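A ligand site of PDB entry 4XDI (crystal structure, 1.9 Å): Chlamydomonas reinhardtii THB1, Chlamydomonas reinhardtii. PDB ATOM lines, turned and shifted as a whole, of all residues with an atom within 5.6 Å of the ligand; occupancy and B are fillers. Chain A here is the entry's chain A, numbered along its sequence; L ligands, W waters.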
ATOM      1  N   LEU A  37      -4.364 -12.692 -31.749  1.00  0.00           N
ATOM      2  CA  LEU A  37      -4.073 -14.107 -31.985  1.00  0.00           C
ATOM      3  C   LEU A  37      -4.633 -14.622 -33.314  1.00  0.00           C
ATOM      4  O   LEU A  37      -4.038 -15.506 -33.941  1.00  0.00           O
ATOM      5  CB  LEU A  37      -4.645 -14.960 -30.826  1.00  0.00           C
ATOM      6  CG  LEU A  37      -4.044 -14.627 -29.461  1.00  0.00           C
ATOM      7  CD1 LEU A  37      -4.872 -15.273 -28.278  1.00  0.00           C
ATOM      8  CD2 LEU A  37      -2.583 -15.115 -29.425  1.00  0.00           C
ATOM      9  N   PHE A  40      -2.391 -15.758 -36.295  1.00  0.00           N
ATOM     10  CA  PHE A  40      -1.681 -17.035 -36.204  1.00  0.00           C
ATOM     11  C   PHE A  40      -2.563 -18.222 -36.529  1.00  0.00           C
ATOM     12  O   PHE A  40      -2.065 -19.305 -36.890  1.00  0.00           O
ATOM     13  CB  PHE A  40      -1.047 -17.187 -34.796  1.00  0.00           C
ATOM     14  CG  PHE A  40       0.010 -16.158 -34.526  1.00  0.00           C
ATOM     15  CD1 PHE A  40      -0.324 -14.929 -33.981  1.00  0.00           C
ATOM     16  CD2 PHE A  40       1.308 -16.377 -34.915  1.00  0.00           C
ATOM     17  CE1 PHE A  40       0.630 -13.951 -33.810  1.00  0.00           C
ATOM     18  CE2 PHE A  40       2.291 -15.394 -34.745  1.00  0.00           C
ATOM     19  CZ  PHE A  40       1.957 -14.182 -34.197  1.00  0.00           C
ATOM     20  N   PHE A  41      -3.870 -18.034 -36.422  1.00  0.00           N
ATOM     21  CA  PHE A  41      -4.845 -19.120 -36.607  1.00  0.00           C
ATOM     22  C   PHE A  41      -5.495 -19.122 -37.992  1.00  0.00           C
ATOM     23  O   PHE A  41      -6.304 -20.001 -38.329  1.00  0.00           O
ATOM     24  CB  PHE A  41      -5.934 -19.026 -35.503  1.00  0.00           C
ATOM     25  CG  PHE A  41      -5.456 -19.529 -34.173  1.00  0.00           C
ATOM     26  CD1 PHE A  41      -4.764 -18.686 -33.311  1.00  0.00           C
ATOM     27  CD2 PHE A  41      -5.625 -20.861 -33.822  1.00  0.00           C
ATOM     28  CE1 PHE A  41      -4.254 -19.182 -32.071  1.00  0.00           C
ATOM     29  CE2 PHE A  41      -5.141 -21.360 -32.568  1.00  0.00           C
ATOM     30  CZ  PHE A  41      -4.470 -20.511 -31.709  1.00  0.00           C
ATOM     31  N   ASN A  43      -4.317 -19.735 -40.911  1.00  0.00           N
ATOM     32  CA  ASN A  43      -3.832 -20.842 -41.723  1.00  0.00           C
ATOM     33  C   ASN A  43      -4.279 -22.230 -41.209  1.00  0.00           C
ATOM     34  O   ASN A  43      -4.067 -23.238 -41.871  1.00  0.00           O
ATOM     35  CB  ASN A  43      -2.294 -20.794 -41.768  1.00  0.00           C
ATOM     36  CG  ASN A  43      -1.709 -21.700 -42.832  1.00  0.00           C
ATOM     37  OD1 ASN A  43      -2.177 -21.721 -43.973  1.00  0.00           O
ATOM     38  ND2 ASN A  43      -0.686 -22.475 -42.456  1.00  0.00           N
ATOM     39  N   VAL A  44      -4.885 -22.282 -40.029  1.00  0.00           N
ATOM     40  CA  VAL A  44      -5.186 -23.569 -39.393  1.00  0.00           C
ATOM     41  C   VAL A  44      -6.465 -24.222 -39.912  1.00  0.00           C
ATOM     42  O   VAL A  44      -7.564 -23.657 -39.782  1.00  0.00           O
ATOM     43  CB  VAL A  44      -5.294 -23.385 -37.863  1.00  0.00           C
ATOM     44  CG1 VAL A  44      -5.616 -24.719 -37.199  1.00  0.00           C
ATOM     45  CG2 VAL A  44      -3.997 -22.794 -37.323  1.00  0.00           C
ATOM     46  N   LYS A  48      -6.651 -29.821 -38.013  1.00  0.00           N
ATOM     47  CA  LYS A  48      -5.636 -29.362 -37.074  1.00  0.00           C
ATOM     48  C   LYS A  48      -6.271 -28.709 -35.850  1.00  0.00           C
ATOM     49  O   LYS A  48      -5.820 -28.919 -34.725  1.00  0.00           O
ATOM     50  CB  LYS A  48      -4.676 -28.398 -37.768  1.00  0.00           C
ATOM     51  CG  LYS A  48      -3.587 -27.860 -36.839  1.00  0.00           C
ATOM     52  CD  LYS A  48      -2.585 -27.006 -37.621  1.00  0.00           C
ATOM     53  CE  LYS A  48      -1.748 -27.854 -38.568  1.00  0.00           C
ATOM     54  NZ  LYS A  48      -1.117 -26.991 -39.626  1.00  0.00           N
ATOM     55  N   ARG A  51      -7.388 -31.421 -33.554  1.00  0.00           N
ATOM     56  CA  ARG A  51      -6.248 -32.007 -32.825  1.00  0.00           C
ATOM     57  C   ARG A  51      -5.777 -31.045 -31.733  1.00  0.00           C
ATOM     58  O   ARG A  51      -5.469 -31.467 -30.624  1.00  0.00           O
ATOM     59  CB  ARG A  51      -5.078 -32.349 -33.767  1.00  0.00           C
ATOM     60  CG  ARG A  51      -5.369 -33.492 -34.742  1.00  0.00           C
ATOM     61  CD  ARG A  51      -4.108 -34.039 -35.406  1.00  0.00           C
ATOM     62  NE  ARG A  51      -3.307 -32.983 -36.015  1.00  0.00           N
ATOM     63  CZ  ARG A  51      -3.432 -32.579 -37.279  1.00  0.00           C
ATOM     64  NH1 ARG A  51      -4.325 -33.147 -38.092  1.00  0.00           N
ATOM     65  NH2 ARG A  51      -2.637 -31.616 -37.753  1.00  0.00           N
ATOM     66  N   LYS A  52      -5.746 -29.750 -32.035  1.00  0.00           N
ATOM     67  CA  LYS A  52      -5.292 -28.776 -31.044  1.00  0.00           C
ATOM     68  C   LYS A  52      -6.230 -28.703 -29.843  1.00  0.00           C
ATOM     69  O   LYS A  52      -5.757 -28.544 -28.712  1.00  0.00           O
ATOM     70  CB  LYS A  52      -5.140 -27.390 -31.659  1.00  0.00           C
ATOM     71  CG  LYS A  52      -4.479 -26.389 -30.726  1.00  0.00           C
ATOM     72  CD  LYS A  52      -3.917 -25.198 -31.525  1.00  0.00           C
ATOM     73  CE  LYS A  52      -3.730 -23.954 -30.689  1.00  0.00           C
ATOM     74  NZ  LYS A  52      -2.874 -24.197 -29.486  1.00  0.00           N
ATOM     75  N   ALA A  55      -5.556 -31.613 -27.705  1.00  0.00           N
ATOM     76  CA  ALA A  55      -4.326 -31.370 -26.954  1.00  0.00           C
ATOM     77  C   ALA A  55      -4.600 -30.483 -25.738  1.00  0.00           C
ATOM     78  O   ALA A  55      -4.137 -30.786 -24.645  1.00  0.00           O
ATOM     79  CB  ALA A  55      -3.250 -30.728 -27.868  1.00  0.00           C
ATOM     80  N   PHE A  56      -5.357 -29.398 -25.925  1.00  0.00           N
ATOM     81  CA  PHE A  56      -5.722 -28.531 -24.800  1.00  0.00           C
ATOM     82  C   PHE A  56      -6.460 -29.323 -23.712  1.00  0.00           C
ATOM     83  O   PHE A  56      -6.146 -29.212 -22.531  1.00  0.00           O
ATOM     84  CB  PHE A  56      -6.629 -27.383 -25.247  1.00  0.00           C
ATOM     85  CG  PHE A  56      -5.889 -26.158 -25.765  1.00  0.00           C
ATOM     86  CD1 PHE A  56      -4.726 -25.703 -25.145  1.00  0.00           C
ATOM     87  CD2 PHE A  56      -6.392 -25.436 -26.845  1.00  0.00           C
ATOM     88  CE1 PHE A  56      -4.066 -24.553 -25.629  1.00  0.00           C
ATOM     89  CE2 PHE A  56      -5.740 -24.279 -27.328  1.00  0.00           C
ATOM     90  CZ  PHE A  56      -4.581 -23.844 -26.718  1.00  0.00           C
ATOM     91  N   TYR A  59      -3.902 -32.042 -22.191  1.00  0.00           N
ATOM     92  CA  TYR A  59      -2.764 -31.417 -21.504  1.00  0.00           C
ATOM     93  C   TYR A  59      -3.213 -30.695 -20.244  1.00  0.00           C
ATOM     94  O   TYR A  59      -2.614 -30.853 -19.180  1.00  0.00           O
ATOM     95  CB  TYR A  59      -2.056 -30.398 -22.408  1.00  0.00           C
ATOM     96  CG  TYR A  59      -0.786 -29.893 -21.757  1.00  0.00           C
ATOM     97  CD1 TYR A  59      -0.804 -28.803 -20.878  1.00  0.00           C
ATOM     98  CD2 TYR A  59       0.430 -30.521 -21.981  1.00  0.00           C
ATOM     99  CE1 TYR A  59       0.340 -28.355 -20.267  1.00  0.00           C
ATOM    100  CE2 TYR A  59       1.589 -30.086 -21.371  1.00  0.00           C
ATOM    101  CZ  TYR A  59       1.542 -28.995 -20.522  1.00  0.00           C
ATOM    102  OH  TYR A  59       2.698 -28.562 -19.926  1.00  0.00           O
ATOM    103  N   VAL A  60      -4.253 -29.886 -20.355  1.00  0.00           N
ATOM    104  CA  VAL A  60      -4.642 -29.052 -19.218  1.00  0.00           C
ATOM    105  C   VAL A  60      -5.450 -29.843 -18.193  1.00  0.00           C
ATOM    106  O   VAL A  60      -5.217 -29.708 -16.988  1.00  0.00           O
ATOM    107  CB  VAL A  60      -5.461 -27.790 -19.678  1.00  0.00           C
ATOM    108  CG1 VAL A  60      -5.966 -27.035 -18.460  1.00  0.00           C
ATOM    109  CG2 VAL A  60      -4.573 -26.896 -20.504  1.00  0.00           C
ATOM    110  N   TYR A  67      -1.665 -36.980 -21.877  1.00  0.00           N
ATOM    111  CA  TYR A  67      -1.541 -35.995 -22.949  1.00  0.00           C
ATOM    112  C   TYR A  67      -1.592 -36.670 -24.317  1.00  0.00           C
ATOM    113  O   TYR A  67      -0.817 -37.570 -24.618  1.00  0.00           O
ATOM    114  CB  TYR A  67      -0.274 -35.166 -22.804  1.00  0.00           C
ATOM    115  CG  TYR A  67      -0.071 -34.270 -24.015  1.00  0.00           C
ATOM    116  CD1 TYR A  67      -1.028 -33.333 -24.362  1.00  0.00           C
ATOM    117  CD2 TYR A  67       1.051 -34.398 -24.840  1.00  0.00           C
ATOM    118  CE1 TYR A  67      -0.876 -32.516 -25.487  1.00  0.00           C
ATOM    119  CE2 TYR A  67       1.217 -33.580 -25.962  1.00  0.00           C
ATOM    120  CZ  TYR A  67       0.249 -32.648 -26.268  1.00  0.00           C
ATOM    121  OH  TYR A  67       0.386 -31.835 -27.388  1.00  0.00           O
ATOM    122  N   GLY A  69      -1.277 -35.672 -28.084  1.00  0.00           N
ATOM    123  CA  GLY A  69      -0.970 -34.691 -29.100  1.00  0.00           C
ATOM    124  C   GLY A  69       0.500 -34.560 -29.385  1.00  0.00           C
ATOM    125  O   GLY A  69       1.330 -35.200 -28.752  1.00  0.00           O
ATOM    126  N   ARG A  70       0.826 -33.711 -30.346  1.00  0.00           N
ATOM    127  CA  ARG A  70       2.208 -33.511 -30.746  1.00  0.00           C
ATOM    128  C   ARG A  70       2.997 -32.814 -29.633  1.00  0.00           C
ATOM    129  O   ARG A  70       2.432 -32.070 -28.828  1.00  0.00           O
ATOM    130  CB  ARG A  70       2.255 -32.717 -32.048  1.00  0.00           C
ATOM    131  CG  ARG A  70       3.629 -32.652 -32.689  1.00  0.00           C
ATOM    132  CD  ARG A  70       3.593 -31.795 -33.936  1.00  0.00           C
ATOM    133  NE  ARG A  70       4.905 -31.649 -34.553  1.00  0.00           N
ATOM    134  CZ  ARG A  70       5.170 -30.763 -35.512  1.00  0.00           C
ATOM    135  NH1 ARG A  70       4.199 -29.949 -35.923  1.00  0.00           N
ATOM    136  NH2 ARG A  70       6.379 -30.683 -36.039  1.00  0.00           N
ATOM    137  N   ASP A  71       4.290 -33.079 -29.576  1.00  0.00           N
ATOM    138  CA  ASP A  71       5.222 -32.373 -28.709  1.00  0.00           C
ATOM    139  C   ASP A  71       5.001 -30.842 -28.822  1.00  0.00           C
ATOM    140  O   ASP A  71       4.883 -30.327 -29.915  1.00  0.00           O
ATOM    141  CB  ASP A  71       6.652 -32.730 -29.108  1.00  0.00           C
ATOM    142  CG  ASP A  71       7.699 -31.999 -28.290  1.00  0.00           C
ATOM    143  OD1 ASP A  71       8.098 -32.542 -27.228  1.00  0.00           O
ATOM    144  OD2 ASP A  71       8.152 -30.912 -28.710  1.00  0.00           O
ATOM    145  N   LEU A  72       4.984 -30.136 -27.685  1.00  0.00           N
ATOM    146  CA  LEU A  72       4.591 -28.714 -27.691  1.00  0.00           C
ATOM    147  C   LEU A  72       5.699 -27.839 -28.275  1.00  0.00           C
ATOM    148  O   LEU A  72       5.427 -26.813 -28.903  1.00  0.00           O
ATOM    149  CB  LEU A  72       4.227 -28.232 -26.286  1.00  0.00           C
ATOM    150  CG  LEU A  72       3.022 -28.861 -25.571  1.00  0.00           C
ATOM    151  CD1 LEU A  72       2.647 -28.017 -24.380  1.00  0.00           C
ATOM    152  CD2 LEU A  72       1.837 -28.997 -26.521  1.00  0.00           C
ATOM    153  N   SER A  75       5.500 -28.293 -32.070  1.00  0.00           N
ATOM    154  CA  SER A  75       4.227 -27.766 -32.576  1.00  0.00           C
ATOM    155  C   SER A  75       4.265 -26.272 -32.846  1.00  0.00           C
ATOM    156  O   SER A  75       3.577 -25.766 -33.738  1.00  0.00           O
ATOM    157  CB  SER A  75       3.088 -28.077 -31.584  1.00  0.00           C
ATOM    158  OG  SER A  75       2.758 -29.450 -31.651  1.00  0.00           O
ATOM    159  N   HIS A  76       5.050 -25.543 -32.063  1.00  0.00           N
ATOM    160  CA  HIS A  76       5.108 -24.078 -32.193  1.00  0.00           C
ATOM    161  C   HIS A  76       6.419 -23.499 -32.675  1.00  0.00           C
ATOM    162  O   HIS A  76       6.590 -22.282 -32.704  1.00  0.00           O
ATOM    163  CB  HIS A  76       4.812 -23.488 -30.831  1.00  0.00           C
ATOM    164  CG  HIS A  76       3.523 -23.968 -30.282  1.00  0.00           C
ATOM    165  ND1 HIS A  76       3.438 -25.102 -29.491  1.00  0.00           N
ATOM    166  CD2 HIS A  76       2.266 -23.510 -30.440  1.00  0.00           C
ATOM    167  CE1 HIS A  76       2.170 -25.291 -29.159  1.00  0.00           C
ATOM    168  NE2 HIS A  76       1.447 -24.347 -29.716  1.00  0.00           N
ATOM    169  N   LEU A  79       6.076 -21.285 -35.759  1.00  0.00           N
ATOM    170  CA  LEU A  79       5.321 -20.081 -35.360  1.00  0.00           C
ATOM    171  C   LEU A  79       6.243 -19.054 -34.737  1.00  0.00           C
ATOM    172  O   LEU A  79       6.131 -17.864 -35.013  1.00  0.00           O
ATOM    173  CB  LEU A  79       4.213 -20.417 -34.371  1.00  0.00           C
ATOM    174  CG  LEU A  79       2.993 -21.175 -34.881  1.00  0.00           C
ATOM    175  CD1 LEU A  79       2.073 -21.453 -33.678  1.00  0.00           C
ATOM    176  CD2 LEU A  79       2.271 -20.334 -35.902  1.00  0.00           C
ATOM    177  N   MET A  85       5.593 -15.543 -33.052  1.00  0.00           N
ATOM    178  CA  MET A  85       4.912 -15.961 -31.820  1.00  0.00           C
ATOM    179  C   MET A  85       5.826 -15.690 -30.623  1.00  0.00           C
ATOM    180  O   MET A  85       7.020 -15.997 -30.681  1.00  0.00           O
ATOM    181  CB  MET A  85       4.554 -17.453 -31.874  1.00  0.00           C
ATOM    182  CG  MET A  85       3.923 -17.982 -30.570  1.00  0.00           C
ATOM    183  SD  MET A  85       3.453 -19.720 -30.694  1.00  0.00           S
ATOM    184  CE  MET A  85       2.920 -20.043 -28.976  1.00  0.00           C
ATOM    185  N   HIS A  89       1.814 -13.588 -26.628  1.00  0.00           N
ATOM    186  CA  HIS A  89       0.728 -14.441 -27.105  1.00  0.00           C
ATOM    187  C   HIS A  89       0.403 -15.527 -26.089  1.00  0.00           C
ATOM    188  O   HIS A  89      -0.759 -15.912 -25.929  1.00  0.00           O
ATOM    189  CB  HIS A  89       1.087 -15.089 -28.421  1.00  0.00           C
ATOM    190  CG  HIS A  89       1.383 -14.096 -29.502  1.00  0.00           C
ATOM    191  ND1 HIS A  89       2.627 -13.978 -30.082  1.00  0.00           N
ATOM    192  CD2 HIS A  89       0.608 -13.149 -30.083  1.00  0.00           C
ATOM    193  CE1 HIS A  89       2.601 -13.030 -31.005  1.00  0.00           C
ATOM    194  NE2 HIS A  89       1.385 -12.508 -31.030  1.00  0.00           N
ATOM    195  N   PHE A  90       1.433 -16.047 -25.424  1.00  0.00           N
ATOM    196  CA  PHE A  90       1.184 -17.041 -24.377  1.00  0.00           C
ATOM    197  C   PHE A  90       0.379 -16.408 -23.254  1.00  0.00           C
ATOM    198  O   PHE A  90      -0.583 -17.018 -22.752  1.00  0.00           O
ATOM    199  CB  PHE A  90       2.510 -17.634 -23.844  1.00  0.00           C
ATOM    200  CG  PHE A  90       2.295 -18.808 -22.923  1.00  0.00           C
ATOM    201  CD1 PHE A  90       2.032 -18.613 -21.577  1.00  0.00           C
ATOM    202  CD2 PHE A  90       2.307 -20.099 -23.411  1.00  0.00           C
ATOM    203  CE1 PHE A  90       1.794 -19.692 -20.718  1.00  0.00           C
ATOM    204  CE2 PHE A  90       2.079 -21.180 -22.562  1.00  0.00           C
ATOM    205  CZ  PHE A  90       1.816 -20.968 -21.219  1.00  0.00           C
ATOM    206  N   VAL A  93      -3.208 -16.171 -24.220  1.00  0.00           N
ATOM    207  CA  VAL A  93      -3.886 -17.470 -24.261  1.00  0.00           C
ATOM    208  C   VAL A  93      -4.155 -17.964 -22.835  1.00  0.00           C
ATOM    209  O   VAL A  93      -5.258 -18.415 -22.509  1.00  0.00           O
ATOM    210  CB  VAL A  93      -3.064 -18.508 -25.054  1.00  0.00           C
ATOM    211  CG1 VAL A  93      -3.630 -19.901 -24.849  1.00  0.00           C
ATOM    212  CG2 VAL A  93      -3.077 -18.134 -26.558  1.00  0.00           C
ATOM    213  N   VAL A 118      -1.553 -24.944 -17.213  1.00  0.00           N
ATOM    214  CA  VAL A 118      -1.289 -24.086 -18.404  1.00  0.00           C
ATOM    215  C   VAL A 118       0.072 -23.436 -18.335  1.00  0.00           C
ATOM    216  O   VAL A 118       0.835 -23.461 -19.306  1.00  0.00           O
ATOM    217  CB  VAL A 118      -2.349 -22.986 -18.560  1.00  0.00           C
ATOM    218  CG1 VAL A 118      -2.054 -22.134 -19.780  1.00  0.00           C
ATOM    219  CG2 VAL A 118      -3.643 -23.615 -18.739  1.00  0.00           C
ATOM    220  N   ALA A 121       3.225 -25.193 -19.552  1.00  0.00           N
ATOM    221  CA  ALA A 121       3.481 -25.286 -20.987  1.00  0.00           C
ATOM    222  C   ALA A 121       4.505 -24.275 -21.468  1.00  0.00           C
ATOM    223  O   ALA A 121       5.133 -24.493 -22.513  1.00  0.00           O
ATOM    224  CB  ALA A 121       2.175 -25.130 -21.777  1.00  0.00           C
ATOM    225  N   ILE A 125       7.214 -24.690 -24.715  1.00  0.00           N
ATOM    226  CA  ILE A 125       7.046 -24.012 -25.993  1.00  0.00           C
ATOM    227  C   ILE A 125       8.239 -23.110 -26.277  1.00  0.00           C
ATOM    228  O   ILE A 125       8.776 -23.092 -27.389  1.00  0.00           O
ATOM    229  CB  ILE A 125       5.742 -23.199 -25.999  1.00  0.00           C
ATOM    230  CG1 ILE A 125       4.531 -24.132 -25.860  1.00  0.00           C
ATOM    231  CG2 ILE A 125       5.645 -22.314 -27.293  1.00  0.00           C
ATOM    232  CD1 ILE A 125       3.150 -23.423 -25.628  1.00  0.00           C
HETATM  233  C1  LIG L   1      -0.526 -25.881 -32.779  1.00  0.00           C
HETATM  234  C2  LIG L   1      -0.972 -27.329 -28.169  1.00  0.00           C
HETATM  235  C3  LIG L   1      -0.222 -22.790 -26.733  1.00  0.00           C
HETATM  236  C4  LIG L   1      -1.063 -21.290 -31.240  1.00  0.00           C
HETATM  237  C5  LIG L   1      -0.598 -26.659 -31.659  1.00  0.00           C
HETATM  238  C6  LIG L   1      -0.473 -28.105 -31.609  1.00  0.00           C
HETATM  239  C7  LIG L   1      -0.605 -28.495 -30.347  1.00  0.00           C
HETATM  240  C8  LIG L   1      -0.791 -27.315 -29.536  1.00  0.00           C
HETATM  241  C9  LIG L   1      -0.526 -29.961 -29.838  1.00  0.00           C
HETATM  242  C10 LIG L   1      -0.248 -29.039 -32.827  1.00  0.00           C
HETATM  243  C11 LIG L   1      -1.605 -29.458 -33.389  1.00  0.00           C
HETATM  244  C12 LIG L   1      -1.475 -30.536 -34.462  1.00  0.00           C
HETATM  245  O1  LIG L   1      -1.624 -31.728 -34.117  1.00  0.00           O
HETATM  246  O2  LIG L   1      -1.249 -30.200 -35.658  1.00  0.00           O
HETATM  247  C13 LIG L   1      -0.831 -26.236 -27.361  1.00  0.00           C
HETATM  248  C14 LIG L   1      -0.910 -26.214 -25.916  1.00  0.00           C
HETATM  249  C15 LIG L   1      -0.695 -24.926 -25.531  1.00  0.00           C
HETATM  250  C16 LIG L   1      -0.502 -24.127 -26.723  1.00  0.00           C
HETATM  251  C17 LIG L   1      -1.207 -27.470 -25.034  1.00  0.00           C
HETATM  252  C18 LIG L   1      -0.683 -24.291 -24.124  1.00  0.00           C
HETATM  253  C19 LIG L   1      -0.965 -24.965 -22.996  1.00  0.00           C
HETATM  254  C20 LIG L   1      -0.369 -21.983 -27.838  1.00  0.00           C
HETATM  255  C21 LIG L   1      -0.291 -20.545 -27.850  1.00  0.00           C
HETATM  256  C22 LIG L   1      -0.500 -20.103 -29.107  1.00  0.00           C
HETATM  257  C23 LIG L   1      -0.758 -21.280 -29.907  1.00  0.00           C
HETATM  258  C24 LIG L   1       0.067 -19.665 -26.634  1.00  0.00           C
HETATM  259  C25 LIG L   1      -0.516 -18.632 -29.552  1.00  0.00           C
HETATM  260  C26 LIG L   1      -0.224 -18.250 -30.810  1.00  0.00           C
HETATM  261  C27 LIG L   1      -1.003 -22.369 -32.057  1.00  0.00           C
HETATM  262  C28 LIG L   1      -1.202 -22.292 -33.492  1.00  0.00           C
HETATM  263  C29 LIG L   1      -1.033 -23.725 -33.975  1.00  0.00           C
HETATM  264  C30 LIG L   1      -0.759 -24.528 -32.799  1.00  0.00           C
HETATM  265  C31 LIG L   1      -1.503 -21.039 -34.337  1.00  0.00           C
HETATM  266  C32 LIG L   1      -1.120 -24.254 -35.417  1.00  0.00           C
HETATM  267  C33 LIG L   1       0.290 -24.188 -35.979  1.00  0.00           C
HETATM  268  C34 LIG L   1       0.259 -24.805 -37.347  1.00  0.00           C
HETATM  269  O3  LIG L   1      -0.380 -24.217 -38.266  1.00  0.00           O
HETATM  270  O4  LIG L   1       0.837 -25.880 -37.523  1.00  0.00           O
HETATM  271  N1  LIG L   1      -0.789 -26.200 -30.369  1.00  0.00           N
HETATM  272  N2  LIG L   1      -0.567 -24.963 -27.808  1.00  0.00           N
HETATM  273  N3  LIG L   1      -0.643 -22.418 -29.122  1.00  0.00           N
HETATM  274  N4  LIG L   1      -0.762 -23.683 -31.705  1.00  0.00           N
HETATM  275 FE1  LIG L   1      -0.676 -24.283 -29.746  1.00  0.00          FE
HETATM  276  O   HOH W   1      -1.602 -32.878 -31.782  1.00  0.00           O
HETATM  277  O   HOH W   2       0.188 -22.063 -39.732  1.00  0.00           O
HETATM  278  O   HOH W   3       3.489 -24.282 -38.149  1.00  0.00           O
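ND1 of His 76 sits at hydrogen-bond distance from O of Leu 72, at 2.7 Å. OH of Tyr 67 lies within hydrogen-bond range of O of Arg 70 (2.5 Å). The backbone carbonyl oxygen of Asp 71 is in hydrogen-bond range of the side-chain hydroxyl of Ser 75. The backbone NH (N) of Ala 121 lies within hydrogen-bond range of the side-chain hydroxyl (OH) of Tyr 59. The backbone carbonyl oxygen (O) of Leu 79 sits at hydrogen-bond distance from the backbone NH (N) of Met 85 (3.1 Å).
Merely in contact with the ligand: Phe 40 (3.1 Å), Phe 41 (3.5 Å), Val 44 (3.7 Å), Ala 55 (3.4 Å), Phe 56 (3.4 Å), Tyr 67 (3.2 Å), Arg 70 (3.8 Å), Leu 72 (3.7 Å), Ser 75 (3.3 Å), Leu 79 (3.4 Å), Met 85 (3.4 Å), His 89 (3.9 Å), Phe 90 (3.6 Å), Val 93 (3.5 Å), Ala 121 (3.4 Å) and Ile 125 (3.6 Å). Hydrophobic or aromatic side chains that line the ligand: Phe 40, Phe 41, Val 44, Ala 55, Phe 56, Leu 72, His 76, Leu 79, Met 85, Phe 90, Val 93, Ala 121 and Ile 125. 20 residues have an atom within 4 Å of the ligand: Phe 40, Phe 41, Val 44, Lys 48, Arg 51, Lys 52, Ala 55, Phe 56, Tyr 67, Arg 70, Leu 72, Ser 75, His 76, Leu 79, Met 85, His 89, Phe 90, Val 93, Ala 121 and Ile 125. The nearest printed residue that does not touch the ligand is Tyr 59 (4.02 Å).
A ring nitrogen (NE2) of His 76 binds an iron atom (FE1) of the ligand (2.1 Å). FE1 of the ligand is bound by NZ of Lys 52, at 2.2 Å. An oxygen (O1) of the ligand is in salt-bridge range of the guanidinium group (NE) of Arg 51 (2.8 Å). An oxygen (O4) of the ligand is in salt-bridge range of the side-chain amino group (NZ) of Lys 48 (3.1 Å).
Water W1 lies within hydrogen-bond range of an oxygen (O1) of the ligand and the backbone NH (N) of Arg 70. Water W2 lies within hydrogen-bond range of O3 of the ligand (2.7 Å) and ND2 of Asn 43 (2.9 Å).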
